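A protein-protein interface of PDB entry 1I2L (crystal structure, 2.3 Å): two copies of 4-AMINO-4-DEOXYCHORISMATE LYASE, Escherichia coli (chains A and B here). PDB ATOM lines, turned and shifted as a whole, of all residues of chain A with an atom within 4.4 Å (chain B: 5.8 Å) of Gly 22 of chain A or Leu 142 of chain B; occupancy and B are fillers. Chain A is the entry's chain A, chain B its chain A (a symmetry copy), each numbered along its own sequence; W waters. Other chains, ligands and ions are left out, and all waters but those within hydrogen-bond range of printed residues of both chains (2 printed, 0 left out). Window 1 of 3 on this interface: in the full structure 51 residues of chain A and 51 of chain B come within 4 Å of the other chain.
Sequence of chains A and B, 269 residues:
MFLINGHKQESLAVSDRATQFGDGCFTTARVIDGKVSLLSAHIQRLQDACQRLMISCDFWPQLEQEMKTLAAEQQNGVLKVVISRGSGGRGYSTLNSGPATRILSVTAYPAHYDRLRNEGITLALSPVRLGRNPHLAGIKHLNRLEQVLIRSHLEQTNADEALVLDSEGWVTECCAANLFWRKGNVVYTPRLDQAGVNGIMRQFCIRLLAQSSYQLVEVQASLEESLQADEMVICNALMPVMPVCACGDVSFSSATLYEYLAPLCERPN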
ATOM      1  N   ARG A  17      -1.559  -6.995  24.756  1.00  0.00           N
ATOM      2  CA  ARG A  17      -0.419  -7.392  25.544  1.00  0.00           C
ATOM      3  C   ARG A  17      -0.533  -8.739  26.250  1.00  0.00           C
ATOM      4  O   ARG A  17       0.481  -9.328  26.633  1.00  0.00           O
ATOM      5  CB  ARG A  17      -0.062  -6.245  26.488  1.00  0.00           C
ATOM      6  CG  ARG A  17       0.430  -5.020  25.683  1.00  0.00           C
ATOM      7  CD  ARG A  17       0.411  -3.775  26.500  1.00  0.00           C
ATOM      8  NE  ARG A  17       1.350  -3.869  27.609  1.00  0.00           N
ATOM      9  CZ  ARG A  17       2.559  -3.322  27.608  1.00  0.00           C
ATOM     10  NH1 ARG A  17       2.970  -2.630  26.546  1.00  0.00           N
ATOM     11  NH2 ARG A  17       3.363  -3.487  28.656  1.00  0.00           N
ATOM     12  N   ALA A  18      -1.752  -9.237  26.430  1.00  0.00           N
ATOM     13  CA  ALA A  18      -1.891 -10.563  27.024  1.00  0.00           C
ATOM     14  C   ALA A  18      -1.181 -11.501  26.030  1.00  0.00           C
ATOM     15  O   ALA A  18      -0.366 -12.336  26.408  1.00  0.00           O
ATOM     16  CB  ALA A  18      -3.348 -10.939  27.158  1.00  0.00           C
ATOM     17  N   THR A  19      -1.474 -11.312  24.753  1.00  0.00           N
ATOM     18  CA  THR A  19      -0.897 -12.117  23.685  1.00  0.00           C
ATOM     19  C   THR A  19       0.624 -11.921  23.520  1.00  0.00           C
ATOM     20  O   THR A  19       1.376 -12.892  23.384  1.00  0.00           O
ATOM     21  CB  THR A  19      -1.617 -11.795  22.358  1.00  0.00           C
ATOM     22  OG1 THR A  19      -3.012 -12.087  22.497  1.00  0.00           O
ATOM     23  CG2 THR A  19      -1.034 -12.594  21.219  1.00  0.00           C
ATOM     24  N   GLN A  20       1.067 -10.668  23.571  1.00  0.00           N
ATOM     25  CA  GLN A  20       2.480 -10.346  23.415  1.00  0.00           C
ATOM     26  C   GLN A  20       3.385 -10.671  24.610  1.00  0.00           C
ATOM     27  O   GLN A  20       4.529 -11.093  24.433  1.00  0.00           O
ATOM     28  CB  GLN A  20       2.653  -8.853  23.087  1.00  0.00           C
ATOM     29  CG  GLN A  20       1.855  -8.361  21.890  1.00  0.00           C
ATOM     30  CD  GLN A  20       2.226  -9.071  20.608  1.00  0.00           C
ATOM     31  OE1 GLN A  20       1.371  -9.335  19.769  1.00  0.00           O
ATOM     32  NE2 GLN A  20       3.504  -9.372  20.441  1.00  0.00           N
ATOM     33  N   PHE A  21       2.898 -10.452  25.827  1.00  0.00           N
ATOM     34  CA  PHE A  21       3.736 -10.701  26.997  1.00  0.00           C
ATOM     35  C   PHE A  21       2.971 -11.316  28.149  1.00  0.00           C
ATOM     36  O   PHE A  21       3.509 -11.370  29.256  1.00  0.00           O
ATOM     37  CB  PHE A  21       4.355  -9.400  27.559  1.00  0.00           C
ATOM     38  CG  PHE A  21       4.753  -8.379  26.527  1.00  0.00           C
ATOM     39  CD1 PHE A  21       5.734  -8.653  25.586  1.00  0.00           C
ATOM     40  CD2 PHE A  21       4.182  -7.104  26.552  1.00  0.00           C
ATOM     41  CE1 PHE A  21       6.150  -7.682  24.684  1.00  0.00           C
ATOM     42  CE2 PHE A  21       4.583  -6.115  25.655  1.00  0.00           C
ATOM     43  CZ  PHE A  21       5.579  -6.401  24.711  1.00  0.00           C
ATOM     44  N   GLY A  22       1.742 -11.766  27.914  1.00  0.00           N
ATOM     45  CA  GLY A  22       0.966 -12.321  29.007  1.00  0.00           C
ATOM     46  C   GLY A  22       0.840 -11.240  30.088  1.00  0.00           C
ATOM     47  O   GLY A  22       0.786 -11.524  31.293  1.00  0.00           O
ATOM     48  N   ASP A  23       0.795  -9.990  29.633  1.00  0.00           N
ATOM     49  CA  ASP A  23       0.715  -8.828  30.496  1.00  0.00           C
ATOM     50  C   ASP A  23      -0.710  -8.621  31.011  1.00  0.00           C
ATOM     51  O   ASP A  23      -1.468  -7.795  30.494  1.00  0.00           O
ATOM     52  CB  ASP A  23       1.212  -7.610  29.711  1.00  0.00           C
ATOM     53  CG  ASP A  23       1.204  -6.328  30.528  1.00  0.00           C
ATOM     54  OD1 ASP A  23       0.985  -6.384  31.745  1.00  0.00           O
ATOM     55  OD2 ASP A  23       1.426  -5.266  29.931  1.00  0.00           O
ATOM     56  N   GLY A  24      -1.059  -9.403  32.026  1.00  0.00           N
ATOM     57  CA  GLY A  24      -2.382  -9.329  32.610  1.00  0.00           C
ATOM     58  C   GLY A  24      -2.580 -10.325  33.732  1.00  0.00           C
ATOM     59  O   GLY A  24      -1.631 -10.932  34.227  1.00  0.00           O
ATOM     60  N   LEU A 142      -0.877 -13.629  34.069  1.00  0.00           N
ATOM     61  CA  LEU A 142      -0.845 -14.490  32.887  1.00  0.00           C
ATOM     62  C   LEU A 142       0.464 -15.178  32.499  1.00  0.00           C
ATOM     63  O   LEU A 142       0.489 -15.920  31.517  1.00  0.00           O
ATOM     64  CB  LEU A 142      -1.379 -13.712  31.687  1.00  0.00           C
ATOM     65  CG  LEU A 142      -2.838 -13.233  31.781  1.00  0.00           C
ATOM     66  CD1 LEU A 142      -3.077 -12.222  30.666  1.00  0.00           C
ATOM     67  CD2 LEU A 142      -3.838 -14.422  31.693  1.00  0.00           C
ATOM     68  N   ASN A 143       1.552 -14.930  33.225  1.00  0.00           N
ATOM     69  CA  ASN A 143       2.817 -15.593  32.904  1.00  0.00           C
ATOM     70  C   ASN A 143       2.782 -16.955  33.602  1.00  0.00           C
ATOM     71  O   ASN A 143       3.300 -17.126  34.706  1.00  0.00           O
ATOM     72  CB  ASN A 143       4.027 -14.789  33.396  1.00  0.00           C
ATOM     73  CG  ASN A 143       4.339 -13.585  32.523  1.00  0.00           C
ATOM     74  OD1 ASN A 143       5.441 -13.042  32.587  1.00  0.00           O
ATOM     75  ND2 ASN A 143       3.371 -13.157  31.711  1.00  0.00           N
ATOM     76  N   ALA B  18      -0.921 -18.147  23.796  1.00  0.00           N
ATOM     77  CA  ALA B  18      -0.062 -16.980  23.968  1.00  0.00           C
ATOM     78  C   ALA B  18      -0.899 -16.013  24.827  1.00  0.00           C
ATOM     79  O   ALA B  18      -0.426 -15.463  25.816  1.00  0.00           O
ATOM     80  CB  ALA B  18       0.264 -16.353  22.632  1.00  0.00           C
ATOM     81  N   THR B  19      -2.160 -15.860  24.454  1.00  0.00           N
ATOM     82  CA  THR B  19      -3.086 -14.978  25.151  1.00  0.00           C
ATOM     83  C   THR B  19      -3.409 -15.438  26.588  1.00  0.00           C
ATOM     84  O   THR B  19      -3.406 -14.633  27.526  1.00  0.00           O
ATOM     85  CB  THR B  19      -4.388 -14.854  24.331  1.00  0.00           C
ATOM     86  OG1 THR B  19      -4.080 -14.321  23.038  1.00  0.00           O
ATOM     87  CG2 THR B  19      -5.384 -13.963  25.031  1.00  0.00           C
ATOM     88  N   PHE B  21      -1.640 -17.799  28.574  1.00  0.00           N
ATOM     89  CA  PHE B  21      -0.516 -17.983  29.488  1.00  0.00           C
ATOM     90  C   PHE B  21       0.795 -17.489  28.916  1.00  0.00           C
ATOM     91  O   PHE B  21       1.843 -17.784  29.493  1.00  0.00           O
ATOM     92  CB  PHE B  21      -0.281 -19.473  29.832  1.00  0.00           C
ATOM     93  CG  PHE B  21      -1.527 -20.306  29.963  1.00  0.00           C
ATOM     94  CD1 PHE B  21      -2.470 -20.040  30.946  1.00  0.00           C
ATOM     95  CD2 PHE B  21      -1.715 -21.414  29.133  1.00  0.00           C
ATOM     96  CE1 PHE B  21      -3.580 -20.858  31.110  1.00  0.00           C
ATOM     97  CE2 PHE B  21      -2.824 -22.247  29.279  1.00  0.00           C
ATOM     98  CZ  PHE B  21      -3.767 -21.972  30.278  1.00  0.00           C
ATOM     99  N   GLY B  22       0.757 -16.759  27.804  1.00  0.00           N
ATOM    100  CA  GLY B  22       1.999 -16.306  27.206  1.00  0.00           C
ATOM    101  C   GLY B  22       2.845 -17.546  26.890  1.00  0.00           C
ATOM    102  O   GLY B  22       4.083 -17.523  26.942  1.00  0.00           O
ATOM    103  N   ASP B  23       2.151 -18.633  26.560  1.00  0.00           N
ATOM    104  CA  ASP B  23       2.764 -19.913  26.263  1.00  0.00           C
ATOM    105  C   ASP B  23       3.340 -19.933  24.847  1.00  0.00           C
ATOM    106  O   ASP B  23       2.730 -20.456  23.911  1.00  0.00           O
ATOM    107  CB  ASP B  23       1.711 -21.008  26.458  1.00  0.00           C
ATOM    108  CG  ASP B  23       2.249 -22.407  26.204  1.00  0.00           C
ATOM    109  OD1 ASP B  23       3.466 -22.571  26.046  1.00  0.00           O
ATOM    110  OD2 ASP B  23       1.433 -23.338  26.170  1.00  0.00           O
ATOM    111  N   GLY B  24       4.518 -19.333  24.711  1.00  0.00           N
ATOM    112  CA  GLY B  24       5.179 -19.261  23.426  1.00  0.00           C
ATOM    113  C   GLY B  24       6.492 -18.512  23.488  1.00  0.00           C
ATOM    114  O   GLY B  24       7.022 -18.231  24.562  1.00  0.00           O
ATOM    115  N   CYS B  25       7.033 -18.197  22.320  1.00  0.00           N
ATOM    116  CA  CYS B  25       8.292 -17.483  22.239  1.00  0.00           C
ATOM    117  C   CYS B  25       8.249 -16.455  21.102  1.00  0.00           C
ATOM    118  O   CYS B  25       7.314 -16.418  20.317  1.00  0.00           O
ATOM    119  CB  CYS B  25       9.420 -18.471  21.994  1.00  0.00           C
ATOM    120  SG  CYS B  25       9.243 -19.347  20.440  1.00  0.00           S
ATOM    121  N   PHE B  26       9.274 -15.626  21.009  1.00  0.00           N
ATOM    122  CA  PHE B  26       9.295 -14.634  19.956  1.00  0.00           C
ATOM    123  C   PHE B  26      10.689 -14.143  19.680  1.00  0.00           C
ATOM    124  O   PHE B  26      11.639 -14.457  20.383  1.00  0.00           O
ATOM    125  CB  PHE B  26       8.417 -13.418  20.325  1.00  0.00           C
ATOM    126  CG  PHE B  26       8.955 -12.581  21.466  1.00  0.00           C
ATOM    127  CD1 PHE B  26       8.882 -13.032  22.779  1.00  0.00           C
ATOM    128  CD2 PHE B  26       9.499 -11.312  21.224  1.00  0.00           C
ATOM    129  CE1 PHE B  26       9.337 -12.232  23.842  1.00  0.00           C
ATOM    130  CE2 PHE B  26       9.953 -10.507  22.270  1.00  0.00           C
ATOM    131  CZ  PHE B  26       9.872 -10.967  23.577  1.00  0.00           C
ATOM    132  N   VAL B  82       6.153 -14.166  16.427  1.00  0.00           N
ATOM    133  CA  VAL B  82       5.684 -14.780  17.647  1.00  0.00           C
ATOM    134  C   VAL B  82       5.246 -16.202  17.336  1.00  0.00           C
ATOM    135  O   VAL B  82       4.562 -16.438  16.332  1.00  0.00           O
ATOM    136  CB  VAL B  82       4.474 -14.031  18.227  1.00  0.00           C
ATOM    137  CG1 VAL B  82       3.881 -14.840  19.367  1.00  0.00           C
ATOM    138  CG2 VAL B  82       4.880 -12.613  18.648  1.00  0.00           C
ATOM    139  N   ILE B  83       5.661 -17.150  18.161  1.00  0.00           N
ATOM    140  CA  ILE B  83       5.210 -18.531  17.955  1.00  0.00           C
ATOM    141  C   ILE B  83       4.603 -18.979  19.271  1.00  0.00           C
ATOM    142  O   ILE B  83       5.223 -18.835  20.314  1.00  0.00           O
ATOM    143  CB  ILE B  83       6.383 -19.501  17.599  1.00  0.00           C
ATOM    144  CG1 ILE B  83       7.003 -19.110  16.263  1.00  0.00           C
ATOM    145  CG2 ILE B  83       5.898 -20.963  17.550  1.00  0.00           C
ATOM    146  CD1 ILE B  83       8.410 -19.668  16.128  1.00  0.00           C
ATOM    147  N   SER B  84       3.384 -19.485  19.244  1.00  0.00           N
ATOM    148  CA  SER B  84       2.792 -19.965  20.494  1.00  0.00           C
ATOM    149  C   SER B  84       2.367 -21.414  20.301  1.00  0.00           C
ATOM    150  O   SER B  84       2.340 -21.899  19.178  1.00  0.00           O
ATOM    151  CB  SER B  84       1.574 -19.120  20.896  1.00  0.00           C
ATOM    152  OG  SER B  84       0.444 -19.493  20.151  1.00  0.00           O
ATOM    153  N   LYS B 140      13.678 -16.602  24.670  1.00  0.00           N
ATOM    154  CA  LYS B 140      12.916 -15.381  24.500  1.00  0.00           C
ATOM    155  C   LYS B 140      11.434 -15.783  24.463  1.00  0.00           C
ATOM    156  O   LYS B 140      10.751 -15.635  23.462  1.00  0.00           O
ATOM    157  CB  LYS B 140      13.339 -14.680  23.216  1.00  0.00           C
ATOM    158  CG  LYS B 140      12.931 -13.216  23.146  1.00  0.00           C
ATOM    159  CD  LYS B 140      13.415 -12.624  21.826  1.00  0.00           C
ATOM    160  CE  LYS B 140      14.012 -11.243  21.982  1.00  0.00           C
ATOM    161  NZ  LYS B 140      13.156 -10.195  21.074  1.00  0.00           N
ATOM    162  N   HIS B 141      10.959 -16.316  25.578  1.00  0.00           N
ATOM    163  CA  HIS B 141       9.572 -16.747  25.710  1.00  0.00           C
ATOM    164  C   HIS B 141       8.662 -15.549  25.975  1.00  0.00           C
ATOM    165  O   HIS B 141       9.138 -14.450  26.276  1.00  0.00           O
ATOM    166  CB  HIS B 141       9.458 -17.766  26.832  1.00  0.00           C
ATOM    167  CG  HIS B 141       9.966 -17.269  28.152  1.00  0.00           C
ATOM    168  ND1 HIS B 141       9.272 -16.363  28.927  1.00  0.00           N
ATOM    169  CD2 HIS B 141      11.106 -17.546  28.828  1.00  0.00           C
ATOM    170  CE1 HIS B 141       9.963 -16.102  30.020  1.00  0.00           C
ATOM    171  NE2 HIS B 141      11.081 -16.808  29.984  1.00  0.00           N
ATOM    172  N   LEU B 142       7.353 -15.773  25.873  1.00  0.00           N
ATOM    173  CA  LEU B 142       6.371 -14.703  26.046  1.00  0.00           C
ATOM    174  C   LEU B 142       6.026 -14.227  27.458  1.00  0.00           C
ATOM    175  O   LEU B 142       5.217 -13.312  27.607  1.00  0.00           O
ATOM    176  CB  LEU B 142       5.086 -15.079  25.314  1.00  0.00           C
ATOM    177  CG  LEU B 142       5.199 -15.261  23.791  1.00  0.00           C
ATOM    178  CD1 LEU B 142       3.925 -15.939  23.300  1.00  0.00           C
ATOM    179  CD2 LEU B 142       5.435 -13.904  23.068  1.00  0.00           C
ATOM    180  N   ASN B 143       6.597 -14.841  28.493  1.00  0.00           N
ATOM    181  CA  ASN B 143       6.315 -14.395  29.858  1.00  0.00           C
ATOM    182  C   ASN B 143       7.276 -13.238  30.143  1.00  0.00           C
ATOM    183  O   ASN B 143       8.345 -13.416  30.726  1.00  0.00           O
ATOM    184  CB  ASN B 143       6.534 -15.515  30.884  1.00  0.00           C
ATOM    185  CG  ASN B 143       5.413 -16.540  30.898  1.00  0.00           C
ATOM    186  OD1 ASN B 143       5.276 -17.295  31.858  1.00  0.00           O
ATOM    187  ND2 ASN B 143       4.612 -16.577  29.832  1.00  0.00           N
ATOM    188  N   ARG B 144       6.891 -12.043  29.717  1.00  0.00           N
ATOM    189  CA  ARG B 144       7.746 -10.897  29.920  1.00  0.00           C
ATOM    190  C   ARG B 144       7.197  -9.842  30.887  1.00  0.00           C
ATOM    191  O   ARG B 144       7.501  -8.653  30.772  1.00  0.00           O
ATOM    192  CB  ARG B 144       8.073 -10.304  28.560  1.00  0.00           C
ATOM    193  CG  ARG B 144       8.622 -11.342  27.569  1.00  0.00           C
ATOM    194  CD  ARG B 144      10.143 -11.384  27.487  1.00  0.00           C
ATOM    195  NE  ARG B 144      10.808 -11.902  28.682  1.00  0.00           N
ATOM    196  CZ  ARG B 144      11.507 -13.037  28.731  1.00  0.00           C
ATOM    197  NH1 ARG B 144      11.634 -13.801  27.655  1.00  0.00           N
ATOM    198  NH2 ARG B 144      12.115 -13.394  29.847  1.00  0.00           N
ATOM    199  N   LEU B 145       6.403 -10.283  31.854  1.00  0.00           N
ATOM    200  CA  LEU B 145       5.849  -9.376  32.854  1.00  0.00           C
ATOM    201  C   LEU B 145       6.982  -8.779  33.671  1.00  0.00           C
ATOM    202  O   LEU B 145       6.914  -7.645  34.112  1.00  0.00           O
ATOM    203  CB  LEU B 145       4.887 -10.115  33.793  1.00  0.00           C
ATOM    204  CG  LEU B 145       3.392  -9.925  33.544  1.00  0.00           C
ATOM    205  CD1 LEU B 145       2.591 -10.787  34.545  1.00  0.00           C
ATOM    206  CD2 LEU B 145       3.036  -8.431  33.667  1.00  0.00           C
HETATM  207  O   HOH W   1       6.693 -17.814  34.226  1.00  0.00           O
HETATM  208  O   HOH W   2       7.742 -13.344  34.167  1.00  0.00           O
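The side-chain hydroxyl of Thr 19 of chain B lies within hydrogen-bond range of the side-chain hydroxyl of Thr 19 of chain A (2.5 Å). The side-chain amide oxygen (OD1) of Asn 143 of chain B sits close to the backbone carbonyl oxygen (O) of Asn 143 of chain A. The backbone carbonyl oxygen (O) of Leu 142 of chain A lies close to the backbone carbonyl oxygen (O) of Phe 21 of chain B (3.1 Å). OD1 of Asn 143 of chain A lies within hydrogen-bond range of N of Leu 145 of chain B, at 3.0 Å. The backbone carbonyl oxygen of Phe 21 of chain A lies within hydrogen-bond range of the backbone NH of Arg 144 of chain B. O of Ala 18 of chain A lies close to O of Ala 18 of chain B (3.2 Å). OD1 of Asn 143 of chain A sits at hydrogen-bond distance from N of Arg 144 of chain B (3.4 Å). O of Phe 21 of chain A lies close to O of Leu 142 of chain B, 3.1 Å away.
The backbone carbonyl oxygen (O) of Gly 22 of chain A sits at hydrogen-bond distance from the side-chain amide nitrogen (ND2) of Asn 143 of chain A, 3.1 Å away. OD2 of Asp 23 of chain A lies within salt-bridge range of NE of Arg 17 of chain A, at 2.7 Å. N of Asn 143 of chain B is in hydrogen-bond range of ND1 of His 141 of chain B. ND2 of Asn 143 of chain B lies within hydrogen-bond range of O of Phe 21 of chain B (3.0 Å). The backbone carbonyl oxygen (O) of Phe 21 of chain A lies within hydrogen-bond range of the side-chain amide nitrogen (ND2) of Asn 143 of chain A, 3.0 Å away. The backbone carbonyl oxygen (O) of Gly 22 of chain B sits at hydrogen-bond distance from the side-chain amide nitrogen (ND2) of Asn 143 of chain B (3.1 Å).
CB of Ala 18 of chain A touches O of Thr 19 of chain B, at 3.7 Å. Thr 19 of chain A touches Ala 18 of chain B (O to CB, 3.7 Å). Leu 142 of chain B touches Thr 19 of chain A (CD1 to O, 3.97 Å). Gln 20 of chain A touches Val 82 of chain B. Leu 142 of chain B touches Gln 20 of chain A. O of Leu 142 of chain B touches N of Gly 22 of chain A (3.8 Å). Gly 22 of chain A touches Leu 145 of chain B. OD1 of Asp 23 of chain A touches CD2 of Leu 145 of chain B, at 3.5 Å. Thr 19 of chain B touches Leu 142 of chain A. O of Leu 142 of chain A touches N of Gly 22 of chain B, at 3.8 Å.
Of chain B, only Leu 142 and Leu 145 come within 4 Å of Gly 22 of chain A. Of chain A, only Thr 19 (3.97 Å), Gln 20 (3.3 Å), Phe 21 (3.1 Å) and Gly 22 (3.8 Å) come within 4 Å of Leu 142 of chain B. Printed residues of chain A within 4 Å of Arg 144 of chain B: Phe 21 and Asn 143. Printed residues of chain B within 4 Å of Gln 20 of chain A: Val 82 and Leu 142. Of the printed residues of chain B, Ala 18 of chain A touches Ala 18 and Thr 19. His 141 of chain B touches none of the printed residues of chain A. Lys 140 of chain B touches none of the printed residues of chain A. The nearest printed residue of chain A that does not touch Arg 144 of chain B is Gln 20 of chain A (5.2 Å).
Printed residues of chain A that touch a printed residue of chain B: Ala 18, Thr 19, Gln 20, Phe 21, Gly 22, Asp 23, Leu 142 and Asn 143. Printed residues of chain B that touch a printed residue of chain A: Ala 18, Thr 19, Phe 21, Gly 22, Val 82, Leu 142, Asn 143, Arg 144 and Leu 145. Among the printed residues, no Asp or Glu carboxylate lies within 4 Å of a Lys or Arg side-chain nitrogen of the other chain.
Ala 18 of chain A touches its own counterpart, Ala 18 of chain B. Thr 19 of chain B touches its own counterpart, Thr 19 of chain A. Phe 21 of chain A touches Leu 142 of chain B, and with the chains exchanged Leu 142 of chain A touches Phe 21 of chain B. Asn 143 of chain B touches its own counterpart, Asn 143 of chain A.
Water W2 lies within hydrogen-bond range of OD1 of Asn 143 of chain A (2.8 Å) and O of Asn 143 of chain B (3.5 Å). Water W1 bridges OD1 of Asn 143 of chain B (2.8 Å) and O of Asn 143 of chain A (3.5 Å).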
